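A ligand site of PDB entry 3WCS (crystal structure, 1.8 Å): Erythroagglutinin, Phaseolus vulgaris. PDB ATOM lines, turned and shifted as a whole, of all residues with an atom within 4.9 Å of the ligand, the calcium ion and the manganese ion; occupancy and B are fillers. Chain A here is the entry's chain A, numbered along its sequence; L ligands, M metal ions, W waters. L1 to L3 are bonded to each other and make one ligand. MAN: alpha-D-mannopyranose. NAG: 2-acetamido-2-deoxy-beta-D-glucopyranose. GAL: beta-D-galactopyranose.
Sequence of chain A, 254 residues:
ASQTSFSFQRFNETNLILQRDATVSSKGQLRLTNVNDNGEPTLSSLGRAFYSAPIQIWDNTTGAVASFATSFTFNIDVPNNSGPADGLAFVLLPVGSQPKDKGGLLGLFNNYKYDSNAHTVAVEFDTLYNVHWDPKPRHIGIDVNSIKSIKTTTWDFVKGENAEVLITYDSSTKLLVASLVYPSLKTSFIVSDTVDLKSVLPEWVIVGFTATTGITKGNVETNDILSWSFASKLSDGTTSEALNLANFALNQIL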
ATOM      1  N   ASP A  86      -7.588 -15.120  27.507  1.00  0.00           N
ATOM      2  CA  ASP A  86      -6.168 -15.550  27.392  1.00  0.00           C
ATOM      3  C   ASP A  86      -5.510 -14.967  26.154  1.00  0.00           C
ATOM      4  O   ASP A  86      -4.265 -14.937  26.040  1.00  0.00           O
ATOM      5  CB  ASP A  86      -6.110 -17.076  27.282  1.00  0.00           C
ATOM      6  CG  ASP A  86      -5.940 -17.740  28.609  1.00  0.00           C
ATOM      7  OD1 ASP A  86      -4.788 -17.729  29.124  1.00  0.00           O
ATOM      8  OD2 ASP A  86      -6.929 -18.319  29.126  1.00  0.00           O
ATOM      9  N   LYS A 102      -8.283 -25.467  25.587  1.00  0.00           N
ATOM     10  CA  LYS A 102      -8.678 -24.080  25.827  1.00  0.00           C
ATOM     11  C   LYS A 102      -7.684 -23.296  26.697  1.00  0.00           C
ATOM     12  O   LYS A 102      -6.515 -23.697  26.870  1.00  0.00           O
ATOM     13  CB  LYS A 102     -10.086 -24.051  26.437  1.00  0.00           C
ATOM     14  CG  LYS A 102     -10.178 -24.694  27.825  1.00  0.00           C
ATOM     15  CD  LYS A 102     -11.574 -24.539  28.434  1.00  0.00           C
ATOM     16  CE  LYS A 102     -12.493 -25.678  28.019  1.00  0.00           C
ATOM     17  NZ  LYS A 102     -13.895 -25.421  28.462  1.00  0.00           N
ATOM     18  N   GLY A 103      -8.131 -22.159  27.222  1.00  0.00           N
ATOM     19  CA  GLY A 103      -7.261 -21.337  28.081  1.00  0.00           C
ATOM     20  C   GLY A 103      -5.969 -20.884  27.398  1.00  0.00           C
ATOM     21  O   GLY A 103      -5.970 -20.423  26.263  1.00  0.00           O
ATOM     22  N   GLY A 104      -4.840 -21.058  28.104  1.00  0.00           N
ATOM     23  CA  GLY A 104      -3.569 -20.569  27.590  1.00  0.00           C
ATOM     24  C   GLY A 104      -3.063 -21.287  26.333  1.00  0.00           C
ATOM     25  O   GLY A 104      -2.134 -20.846  25.701  1.00  0.00           O
ATOM     26  N   LEU A 105      -3.667 -22.406  25.994  1.00  0.00           N
ATOM     27  CA  LEU A 105      -3.269 -23.117  24.787  1.00  0.00           C
ATOM     28  C   LEU A 105      -4.033 -22.619  23.541  1.00  0.00           C
ATOM     29  O   LEU A 105      -3.774 -23.073  22.414  1.00  0.00           O
ATOM     30  CB  LEU A 105      -3.441 -24.622  25.001  1.00  0.00           C
ATOM     31  CG  LEU A 105      -2.531 -25.179  26.124  1.00  0.00           C
ATOM     32  CD1 LEU A 105      -2.862 -26.633  26.454  1.00  0.00           C
ATOM     33  CD2 LEU A 105      -1.055 -24.987  25.800  1.00  0.00           C
ATOM     34  N   TYR A 112       2.131 -27.890  26.146  1.00  0.00           N
ATOM     35  CA  TYR A 112       3.076 -26.842  25.759  1.00  0.00           C
ATOM     36  C   TYR A 112       4.404 -27.340  25.169  1.00  0.00           C
ATOM     37  O   TYR A 112       5.381 -26.599  25.127  1.00  0.00           O
ATOM     38  CB  TYR A 112       3.299 -25.831  26.892  1.00  0.00           C
ATOM     39  CG  TYR A 112       3.699 -26.386  28.253  1.00  0.00           C
ATOM     40  CD1 TYR A 112       5.043 -26.492  28.627  1.00  0.00           C
ATOM     41  CD2 TYR A 112       2.727 -26.747  29.187  1.00  0.00           C
ATOM     42  CE1 TYR A 112       5.408 -26.974  29.889  1.00  0.00           C
ATOM     43  CE2 TYR A 112       3.074 -27.217  30.454  1.00  0.00           C
ATOM     44  CZ  TYR A 112       4.411 -27.334  30.790  1.00  0.00           C
ATOM     45  OH  TYR A 112       4.717 -27.796  32.053  1.00  0.00           O
ATOM     46  N   GLU A 124       0.070 -14.762  17.631  1.00  0.00           N
ATOM     47  CA  GLU A 124      -0.720 -14.648  18.853  1.00  0.00           C
ATOM     48  C   GLU A 124      -0.626 -13.285  19.509  1.00  0.00           C
ATOM     49  O   GLU A 124       0.402 -12.604  19.419  1.00  0.00           O
ATOM     50  CB  GLU A 124      -0.343 -15.725  19.875  1.00  0.00           C
ATOM     51  CG  GLU A 124       1.113 -15.634  20.395  1.00  0.00           C
ATOM     52  CD  GLU A 124       1.352 -16.472  21.659  1.00  0.00           C
ATOM     53  OE1 GLU A 124       1.035 -17.692  21.590  1.00  0.00           O
ATOM     54  OE2 GLU A 124       1.836 -15.960  22.723  1.00  0.00           O
ATOM     55  N   ASP A 126      -1.243 -12.266  23.080  1.00  0.00           N
ATOM     56  CA  ASP A 126      -1.335 -13.076  24.334  1.00  0.00           C
ATOM     57  C   ASP A 126      -1.426 -12.113  25.524  1.00  0.00           C
ATOM     58  O   ASP A 126      -0.517 -11.312  25.760  1.00  0.00           O
ATOM     59  CB  ASP A 126      -0.074 -13.990  24.419  1.00  0.00           C
ATOM     60  CG  ASP A 126      -0.125 -15.043  25.552  1.00  0.00           C
ATOM     61  OD1 ASP A 126      -0.990 -14.888  26.436  1.00  0.00           O
ATOM     62  OD2 ASP A 126       0.704 -16.043  25.544  1.00  0.00           O
ATOM     63  N   LEU A 128      -2.191 -13.075  28.798  1.00  0.00           N
ATOM     64  CA  LEU A 128      -2.048 -13.764  30.092  1.00  0.00           C
ATOM     65  C   LEU A 128      -0.721 -14.517  30.151  1.00  0.00           C
ATOM     66  O   LEU A 128      -0.441 -15.394  29.343  1.00  0.00           O
ATOM     67  CB  LEU A 128      -3.214 -14.728  30.338  1.00  0.00           C
ATOM     68  CG  LEU A 128      -3.028 -15.209  31.802  1.00  0.00           C
ATOM     69  CD1 LEU A 128      -4.107 -14.803  32.800  1.00  0.00           C
ATOM     70  CD2 LEU A 128      -2.509 -16.649  31.906  1.00  0.00           C
ATOM     71  N   TYR A 129       0.074 -14.161  31.161  1.00  0.00           N
ATOM     72  CA  TYR A 129       1.378 -14.830  31.391  1.00  0.00           C
ATOM     73  C   TYR A 129       1.209 -16.258  31.899  1.00  0.00           C
ATOM     74  O   TYR A 129       0.697 -16.476  33.012  1.00  0.00           O
ATOM     75  CB  TYR A 129       2.146 -13.988  32.393  1.00  0.00           C
ATOM     76  CG  TYR A 129       3.330 -14.680  33.067  1.00  0.00           C
ATOM     77  CD1 TYR A 129       4.365 -15.185  32.320  1.00  0.00           C
ATOM     78  CD2 TYR A 129       3.354 -14.844  34.442  1.00  0.00           C
ATOM     79  CE1 TYR A 129       5.455 -15.805  32.960  1.00  0.00           C
ATOM     80  CE2 TYR A 129       4.422 -15.459  35.091  1.00  0.00           C
ATOM     81  CZ  TYR A 129       5.457 -15.940  34.344  1.00  0.00           C
ATOM     82  OH  TYR A 129       6.519 -16.560  35.005  1.00  0.00           O
ATOM     83  N   ASN A 130       1.646 -17.231  31.093  1.00  0.00           N
ATOM     84  CA  ASN A 130       1.542 -18.634  31.461  1.00  0.00           C
ATOM     85  C   ASN A 130       2.947 -19.033  31.879  1.00  0.00           C
ATOM     86  O   ASN A 130       3.858 -19.073  31.066  1.00  0.00           O
ATOM     87  CB  ASN A 130       1.046 -19.480  30.281  1.00  0.00           C
ATOM     88  CG  ASN A 130      -0.445 -19.295  30.021  1.00  0.00           C
ATOM     89  OD1 ASN A 130      -0.850 -18.598  29.068  1.00  0.00           O
ATOM     90  ND2 ASN A 130      -1.264 -19.935  30.865  1.00  0.00           N
ATOM     91  N   VAL A 131       3.108 -19.280  33.174  1.00  0.00           N
ATOM     92  CA  VAL A 131       4.440 -19.448  33.784  1.00  0.00           C
ATOM     93  C   VAL A 131       5.367 -20.456  33.116  1.00  0.00           C
ATOM     94  O   VAL A 131       6.595 -20.284  33.113  1.00  0.00           O
ATOM     95  CB  VAL A 131       4.279 -19.752  35.305  1.00  0.00           C
ATOM     96  CG1 VAL A 131       3.551 -21.071  35.532  1.00  0.00           C
ATOM     97  CG2 VAL A 131       5.625 -19.741  36.010  1.00  0.00           C
ATOM     98  N   HIS A 132       4.803 -21.506  32.539  1.00  0.00           N
ATOM     99  CA  HIS A 132       5.635 -22.593  31.990  1.00  0.00           C
ATOM    100  C   HIS A 132       6.209 -22.338  30.622  1.00  0.00           C
ATOM    101  O   HIS A 132       7.076 -23.087  30.143  1.00  0.00           O
ATOM    102  CB  HIS A 132       4.888 -23.924  32.026  1.00  0.00           C
ATOM    103  CG  HIS A 132       4.485 -24.362  33.414  1.00  0.00           C
ATOM    104  ND1 HIS A 132       5.380 -24.535  34.420  1.00  0.00           N
ATOM    105  CD2 HIS A 132       3.235 -24.728  33.929  1.00  0.00           C
ATOM    106  CE1 HIS A 132       4.741 -24.938  35.535  1.00  0.00           C
ATOM    107  NE2 HIS A 132       3.419 -25.065  35.242  1.00  0.00           N
ATOM    108  N   TRP A 133       5.750 -21.275  29.943  1.00  0.00           N
ATOM    109  CA  TRP A 133       6.252 -20.971  28.595  1.00  0.00           C
ATOM    110  C   TRP A 133       6.335 -19.536  28.136  1.00  0.00           C
ATOM    111  O   TRP A 133       7.083 -19.235  27.233  1.00  0.00           O
ATOM    112  CB  TRP A 133       5.507 -21.808  27.548  1.00  0.00           C
ATOM    113  CG  TRP A 133       4.057 -21.403  27.399  1.00  0.00           C
ATOM    114  CD1 TRP A 133       3.554 -20.344  26.655  1.00  0.00           C
ATOM    115  CD2 TRP A 133       2.894 -22.078  27.954  1.00  0.00           C
ATOM    116  NE1 TRP A 133       2.170 -20.294  26.752  1.00  0.00           N
ATOM    117  CE2 TRP A 133       1.714 -21.318  27.501  1.00  0.00           C
ATOM    118  CE3 TRP A 133       2.697 -23.185  28.779  1.00  0.00           C
ATOM    119  CZ2 TRP A 133       0.436 -21.675  27.859  1.00  0.00           C
ATOM    120  CZ3 TRP A 133       1.401 -23.535  29.133  1.00  0.00           C
ATOM    121  CH2 TRP A 133       0.293 -22.786  28.687  1.00  0.00           C
ATOM    122  N   ASP A 134       5.536 -18.636  28.713  1.00  0.00           N
ATOM    123  CA  ASP A 134       5.468 -17.247  28.238  1.00  0.00           C
ATOM    124  C   ASP A 134       6.520 -16.311  28.856  1.00  0.00           C
ATOM    125  O   ASP A 134       6.884 -16.499  30.009  1.00  0.00           O
ATOM    126  CB  ASP A 134       4.095 -16.642  28.594  1.00  0.00           C
ATOM    127  CG  ASP A 134       2.991 -16.993  27.574  1.00  0.00           C
ATOM    128  OD1 ASP A 134       3.241 -17.105  26.328  1.00  0.00           O
ATOM    129  OD2 ASP A 134       1.829 -17.076  28.064  1.00  0.00           O
ATOM    130  N   PRO A 135       6.935 -15.251  28.111  1.00  0.00           N
ATOM    131  CA  PRO A 135       7.573 -14.091  28.729  1.00  0.00           C
ATOM    132  C   PRO A 135       6.537 -13.410  29.628  1.00  0.00           C
ATOM    133  O   PRO A 135       5.336 -13.524  29.376  1.00  0.00           O
ATOM    134  CB  PRO A 135       7.944 -13.197  27.543  1.00  0.00           C
ATOM    135  CG  PRO A 135       7.017 -13.595  26.439  1.00  0.00           C
ATOM    136  CD  PRO A 135       6.630 -15.025  26.669  1.00  0.00           C
ATOM    137  N   HIS A 139       2.312  -9.843  25.079  1.00  0.00           N
ATOM    138  CA  HIS A 139       3.203  -9.969  23.930  1.00  0.00           C
ATOM    139  C   HIS A 139       2.485 -10.356  22.662  1.00  0.00           C
ATOM    140  O   HIS A 139       1.395 -10.955  22.694  1.00  0.00           O
ATOM    141  CB  HIS A 139       4.326 -11.003  24.241  1.00  0.00           C
ATOM    142  CG  HIS A 139       3.831 -12.357  24.709  1.00  0.00           C
ATOM    143  ND1 HIS A 139       3.482 -12.602  25.990  1.00  0.00           N
ATOM    144  CD2 HIS A 139       3.575 -13.537  23.989  1.00  0.00           C
ATOM    145  CE1 HIS A 139       3.073 -13.888  26.102  1.00  0.00           C
ATOM    146  NE2 HIS A 139       3.107 -14.476  24.864  1.00  0.00           N
ATOM    147  N   ILE A 147       2.930 -23.681  21.445  1.00  0.00           N
ATOM    148  CA  ILE A 147       2.483 -22.488  22.185  1.00  0.00           C
ATOM    149  C   ILE A 147       3.686 -21.673  22.685  1.00  0.00           C
ATOM    150  O   ILE A 147       3.550 -20.500  23.037  1.00  0.00           O
ATOM    151  CB  ILE A 147       1.502 -22.837  23.334  1.00  0.00           C
ATOM    152  CG1 ILE A 147       0.689 -21.610  23.777  1.00  0.00           C
ATOM    153  CG2 ILE A 147       2.267 -23.372  24.552  1.00  0.00           C
ATOM    154  CD1 ILE A 147      -0.320 -21.107  22.742  1.00  0.00           C
ATOM    155  N   SER A 149       6.329 -19.515  21.759  1.00  0.00           N
ATOM    156  CA  SER A 149       6.560 -18.741  20.514  1.00  0.00           C
ATOM    157  C   SER A 149       8.009 -18.802  20.105  1.00  0.00           C
ATOM    158  O   SER A 149       8.873 -18.738  20.973  1.00  0.00           O
ATOM    159  CB  SER A 149       6.174 -17.280  20.710  1.00  0.00           C
ATOM    160  OG  SER A 149       4.815 -17.197  21.111  1.00  0.00           O
ATOM    161  N   GLY A 214     -10.075 -16.882  30.033  1.00  0.00           N
ATOM    162  CA  GLY A 214      -9.428 -17.520  31.173  1.00  0.00           C
ATOM    163  C   GLY A 214     -10.310 -18.584  31.799  1.00  0.00           C
ATOM    164  O   GLY A 214     -11.544 -18.507  31.724  1.00  0.00           O
ATOM    165  N   ILE A 215      -9.694 -19.580  32.408  1.00  0.00           N
ATOM    166  CA  ILE A 215     -10.474 -20.627  33.062  1.00  0.00           C
ATOM    167  C   ILE A 215     -10.752 -20.317  34.536  1.00  0.00           C
ATOM    168  O   ILE A 215     -11.599 -20.952  35.159  1.00  0.00           O
ATOM    169  CB  ILE A 215      -9.866 -22.033  32.878  1.00  0.00           C
ATOM    170  CG1 ILE A 215      -8.491 -22.160  33.580  1.00  0.00           C
ATOM    171  CG2 ILE A 215      -9.735 -22.374  31.403  1.00  0.00           C
ATOM    172  CD1 ILE A 215      -8.027 -23.601  33.727  1.00  0.00           C
ATOM    173  N   THR A 216     -10.040 -19.327  35.078  1.00  0.00           N
ATOM    174  CA  THR A 216     -10.116 -18.969  36.493  1.00  0.00           C
ATOM    175  C   THR A 216     -10.773 -17.605  36.660  1.00  0.00           C
ATOM    176  O   THR A 216     -10.381 -16.635  35.988  1.00  0.00           O
ATOM    177  CB  THR A 216      -8.706 -18.907  37.112  1.00  0.00           C
ATOM    178  OG1 THR A 216      -8.076 -20.182  36.948  1.00  0.00           O
ATOM    179  CG2 THR A 216      -8.769 -18.566  38.589  1.00  0.00           C
ATOM    180  N   ASN A 219      -9.979 -13.599  35.298  1.00  0.00           N
ATOM    181  CA  ASN A 219      -9.150 -13.599  34.081  1.00  0.00           C
ATOM    182  C   ASN A 219     -10.054 -13.890  32.887  1.00  0.00           C
ATOM    183  O   ASN A 219     -10.367 -15.036  32.599  1.00  0.00           O
ATOM    184  CB  ASN A 219      -8.067 -14.686  34.163  1.00  0.00           C
ATOM    185  CG  ASN A 219      -7.211 -14.550  35.414  1.00  0.00           C
ATOM    186  OD1 ASN A 219      -6.239 -13.797  35.421  1.00  0.00           O
ATOM    187  ND2 ASN A 219      -7.591 -15.252  36.471  1.00  0.00           N
HETATM  188  C1  MAN L   1      -3.848 -23.960  33.604  1.00  0.00           C
HETATM  189  C2  MAN L   1      -4.402 -22.706  32.936  1.00  0.00           C
HETATM  190  C3  MAN L   1      -4.590 -22.973  31.431  1.00  0.00           C
HETATM  191  C4  MAN L   1      -3.254 -23.369  30.807  1.00  0.00           C
HETATM  192  C5  MAN L   1      -2.754 -24.620  31.526  1.00  0.00           C
HETATM  193  C6  MAN L   1      -1.410 -25.122  31.005  1.00  0.00           C
HETATM  194  O1  MAN L   1      -4.807 -24.999  33.571  1.00  0.00           O
HETATM  195  O2  MAN L   1      -3.467 -21.656  33.051  1.00  0.00           O
HETATM  196  O3  MAN L   1      -5.064 -21.784  30.827  1.00  0.00           O
HETATM  197  O4  MAN L   1      -3.363 -23.586  29.402  1.00  0.00           O
HETATM  198  O5  MAN L   1      -2.640 -24.345  32.928  1.00  0.00           O
HETATM  199  O6  MAN L   1      -1.156 -26.407  31.558  1.00  0.00           O
HETATM  200  C1  NAG L   2      -3.726 -20.817  34.194  1.00  0.00           C
HETATM  201  C2  NAG L   2      -2.377 -20.266  34.661  1.00  0.00           C
HETATM  202  C3  NAG L   2      -2.593 -19.316  35.832  1.00  0.00           C
HETATM  203  C4  NAG L   2      -3.627 -18.236  35.515  1.00  0.00           C
HETATM  204  C5  NAG L   2      -4.911 -18.881  34.971  1.00  0.00           C
HETATM  205  C6  NAG L   2      -5.915 -17.849  34.467  1.00  0.00           C
HETATM  206  C7  NAG L   2      -0.499 -21.813  34.363  1.00  0.00           C
HETATM  207  C8  NAG L   2       0.245 -22.987  34.945  1.00  0.00           C
HETATM  208  N2  NAG L   2      -1.537 -21.385  35.067  1.00  0.00           N
HETATM  209  O3  NAG L   2      -1.363 -18.729  36.203  1.00  0.00           O
HETATM  210  O4  NAG L   2      -3.886 -17.577  36.748  1.00  0.00           O
HETATM  211  O5  NAG L   2      -4.608 -19.744  33.883  1.00  0.00           O
HETATM  212  O6  NAG L   2      -7.075 -18.541  34.024  1.00  0.00           O
HETATM  213  O7  NAG L   2      -0.138 -21.315  33.287  1.00  0.00           O
HETATM  214  C1  GAL L   3      -3.747 -16.163  36.650  1.00  0.00           C
HETATM  215  C2  GAL L   3      -4.062 -15.583  38.026  1.00  0.00           C
HETATM  216  C3  GAL L   3      -3.791 -14.082  38.013  1.00  0.00           C
HETATM  217  C4  GAL L   3      -2.384 -13.788  37.501  1.00  0.00           C
HETATM  218  C5  GAL L   3      -2.149 -14.442  36.134  1.00  0.00           C
HETATM  219  C6  GAL L   3      -0.705 -14.331  35.638  1.00  0.00           C
HETATM  220  O2  GAL L   3      -5.398 -15.892  38.394  1.00  0.00           O
HETATM  221  O3  GAL L   3      -3.947 -13.557  39.319  1.00  0.00           O
HETATM  222  O4  GAL L   3      -1.447 -14.340  38.414  1.00  0.00           O
HETATM  223  O5  GAL L   3      -2.432 -15.817  36.255  1.00  0.00           O
HETATM  224  O6  GAL L   3      -0.307 -13.012  35.391  1.00  0.00           O
HETATM  225 CA    CA M   1      -0.413 -16.886  27.521  1.00  0.00          CA
HETATM  226 MN    MN M   2       2.479 -16.388  24.603  1.00  0.00          MN
HETATM  227  O   HOH W   1      -7.000 -19.765  31.527  1.00  0.00           O
HETATM  228  O   HOH W   2       1.815 -18.162  24.081  1.00  0.00           O
HETATM  229  O   HOH W   3       4.296 -16.939  23.971  1.00  0.00           O
HETATM  230  O   HOH W   4      -5.396 -25.280  28.812  1.00  0.00           O
HETATM  231  O   HOH W   5       1.031 -18.304  35.033  1.00  0.00           O
HETATM  232  O   HOH W   6      -0.690 -11.926  32.909  1.00  0.00           O
HETATM  233  O   HOH W   7      -0.256 -18.565  25.906  1.00  0.00           O
HETATM  234  O   HOH W   8       0.422 -26.696  33.836  1.00  0.00           O
HETATM  235  O   HOH W   9      -2.145 -22.608  37.564  1.00  0.00           O
HETATM  236  O   HOH W  10      -0.489 -28.104  29.416  1.00  0.00           O
HETATM  237  O   HOH W  11       2.061 -22.325  32.070  1.00  0.00           O
HETATM  238  O   HOH W  12      -0.646 -17.018  38.427  1.00  0.00           O
HETATM  239  O   HOH W  13      -3.889 -19.359  30.962  1.00  0.00           O
HETATM  240  O   HOH W  14      -2.709 -16.795  27.327  1.00  0.00           O
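Within 4 Å of the calcium ion: Asp 126, Leu 128, Asn 130 and Asp 134. The nearest printed residue that does not touch the calcium ion is Trp 133 (4.3 Å).
The manganese ion is bound by water W2 (2.0 Å), water W3 (2.0 Å), the side-chain carboxylate of Asp 134 (2.0 Å), a ring nitrogen (NE2) of His 139 (2.0 Å), the side-chain carboxylate of Glu 124 (2.0 Å) and the side-chain carboxylate of Asp 126 (2.0 Å). The manganese ion has six donor atoms within binding distance.
N of Gly 104 lies within hydrogen-bond range of O3 of MAN L1 (2.8 Å). An oxygen (O6) of NAG L2 sits at hydrogen-bond distance from the side-chain hydroxyl (OG1) of Thr 216 (3.5 Å). The backbone NH (N) of Thr 216 is in hydrogen-bond range of an oxygen (O6) of NAG L2 (3.2 Å). An oxygen (O7) of NAG L2 is in hydrogen-bond range of the side-chain amide nitrogen (ND2) of Asn 130 (3.0 Å). N of Ile 215 is in hydrogen-bond range of O6 of NAG L2 (3.2 Å). An oxygen (O2) of GAL L3 lies within hydrogen-bond range of the side-chain amide nitrogen (ND2) of Asn 219 (3.0 Å).
Water W7 lies within hydrogen-bond range of O of Gly 104 (3.0 Å) and NE1 of Trp 133 (3.1 Å). Water W2 lies within hydrogen-bond range of OE1 of Glu 124, O of Ile 147 and NE1 of Trp 133. Water W13 lies within hydrogen-bond range of the side-chain carboxylate (OD1) of Asp 86 (2.6 Å), the side-chain amide nitrogen (ND2) of Asn 130 (2.7 Å), an oxygen (O3) of MAN L1 (2.7 Å) and the backbone NH (N) of Gly 104 (3.5 Å). Water W4 bridges an oxygen (O4) of MAN L1 and the backbone carbonyl oxygen (O) of Lys 102. Water W6 bridges O6 of GAL L3 (2.7 Å) and N of Tyr 129 (2.9 Å). Water W1 lies within hydrogen-bond range of an oxygen (O6) of NAG L2, the side-chain carboxylate (OD2) of Asp 86 and the backbone NH (N) of Ile 215.
The indole nitrogen (NE1) of Trp 133 lies close to the side-chain carboxylate (OD1) of Asp 134 (3.4 Å). ND2 of Asn 219 is in hydrogen-bond range of O of Thr 216. O of Asn 219 sits close to N of Gly 214 (3.2 Å). The side-chain carboxylate (OD1) of Asp 86 sits close to the backbone NH (N) of Gly 104, at 3.5 Å.
The calcium ion is bound by water W14 (2.3 Å), the side-chain carboxylate (OD2) of Asp 134 (2.3 Å), water W7 (2.3 Å), the side-chain carboxylate (OD1) of Asp 126 (2.3 Å), the side-chain amide oxygen (OD1) of Asn 130 (2.3 Å), the backbone carbonyl oxygen (O) of Leu 128 (2.4 Å) and the side-chain carboxylate (OD2) of Asp 126 (2.4 Å). The calcium ion has seven donor atoms within binding distance.
The nearest printed residue that does not touch the manganese ion is Ser 149 (4.3 Å).
Gly 103 touches the ligand. N of Leu 105 touches O4 of MAN L1, 3.6 Å away. O of Tyr 129 touches C6 of GAL L3, 3.7 Å away. Val 131 touches the ligand. CD2 of His 132 touches C8 of NAG L2 (3.6 Å). CH2 of Trp 133 touches C6 of MAN L1, at 3.7 Å. Gly 214 touches the ligand. Hydrophobic or aromatic side chains within 4 Å of the ligand: Leu 105, Leu 128, Tyr 129, Val 131, His 132, Trp 133 and Ile 215.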
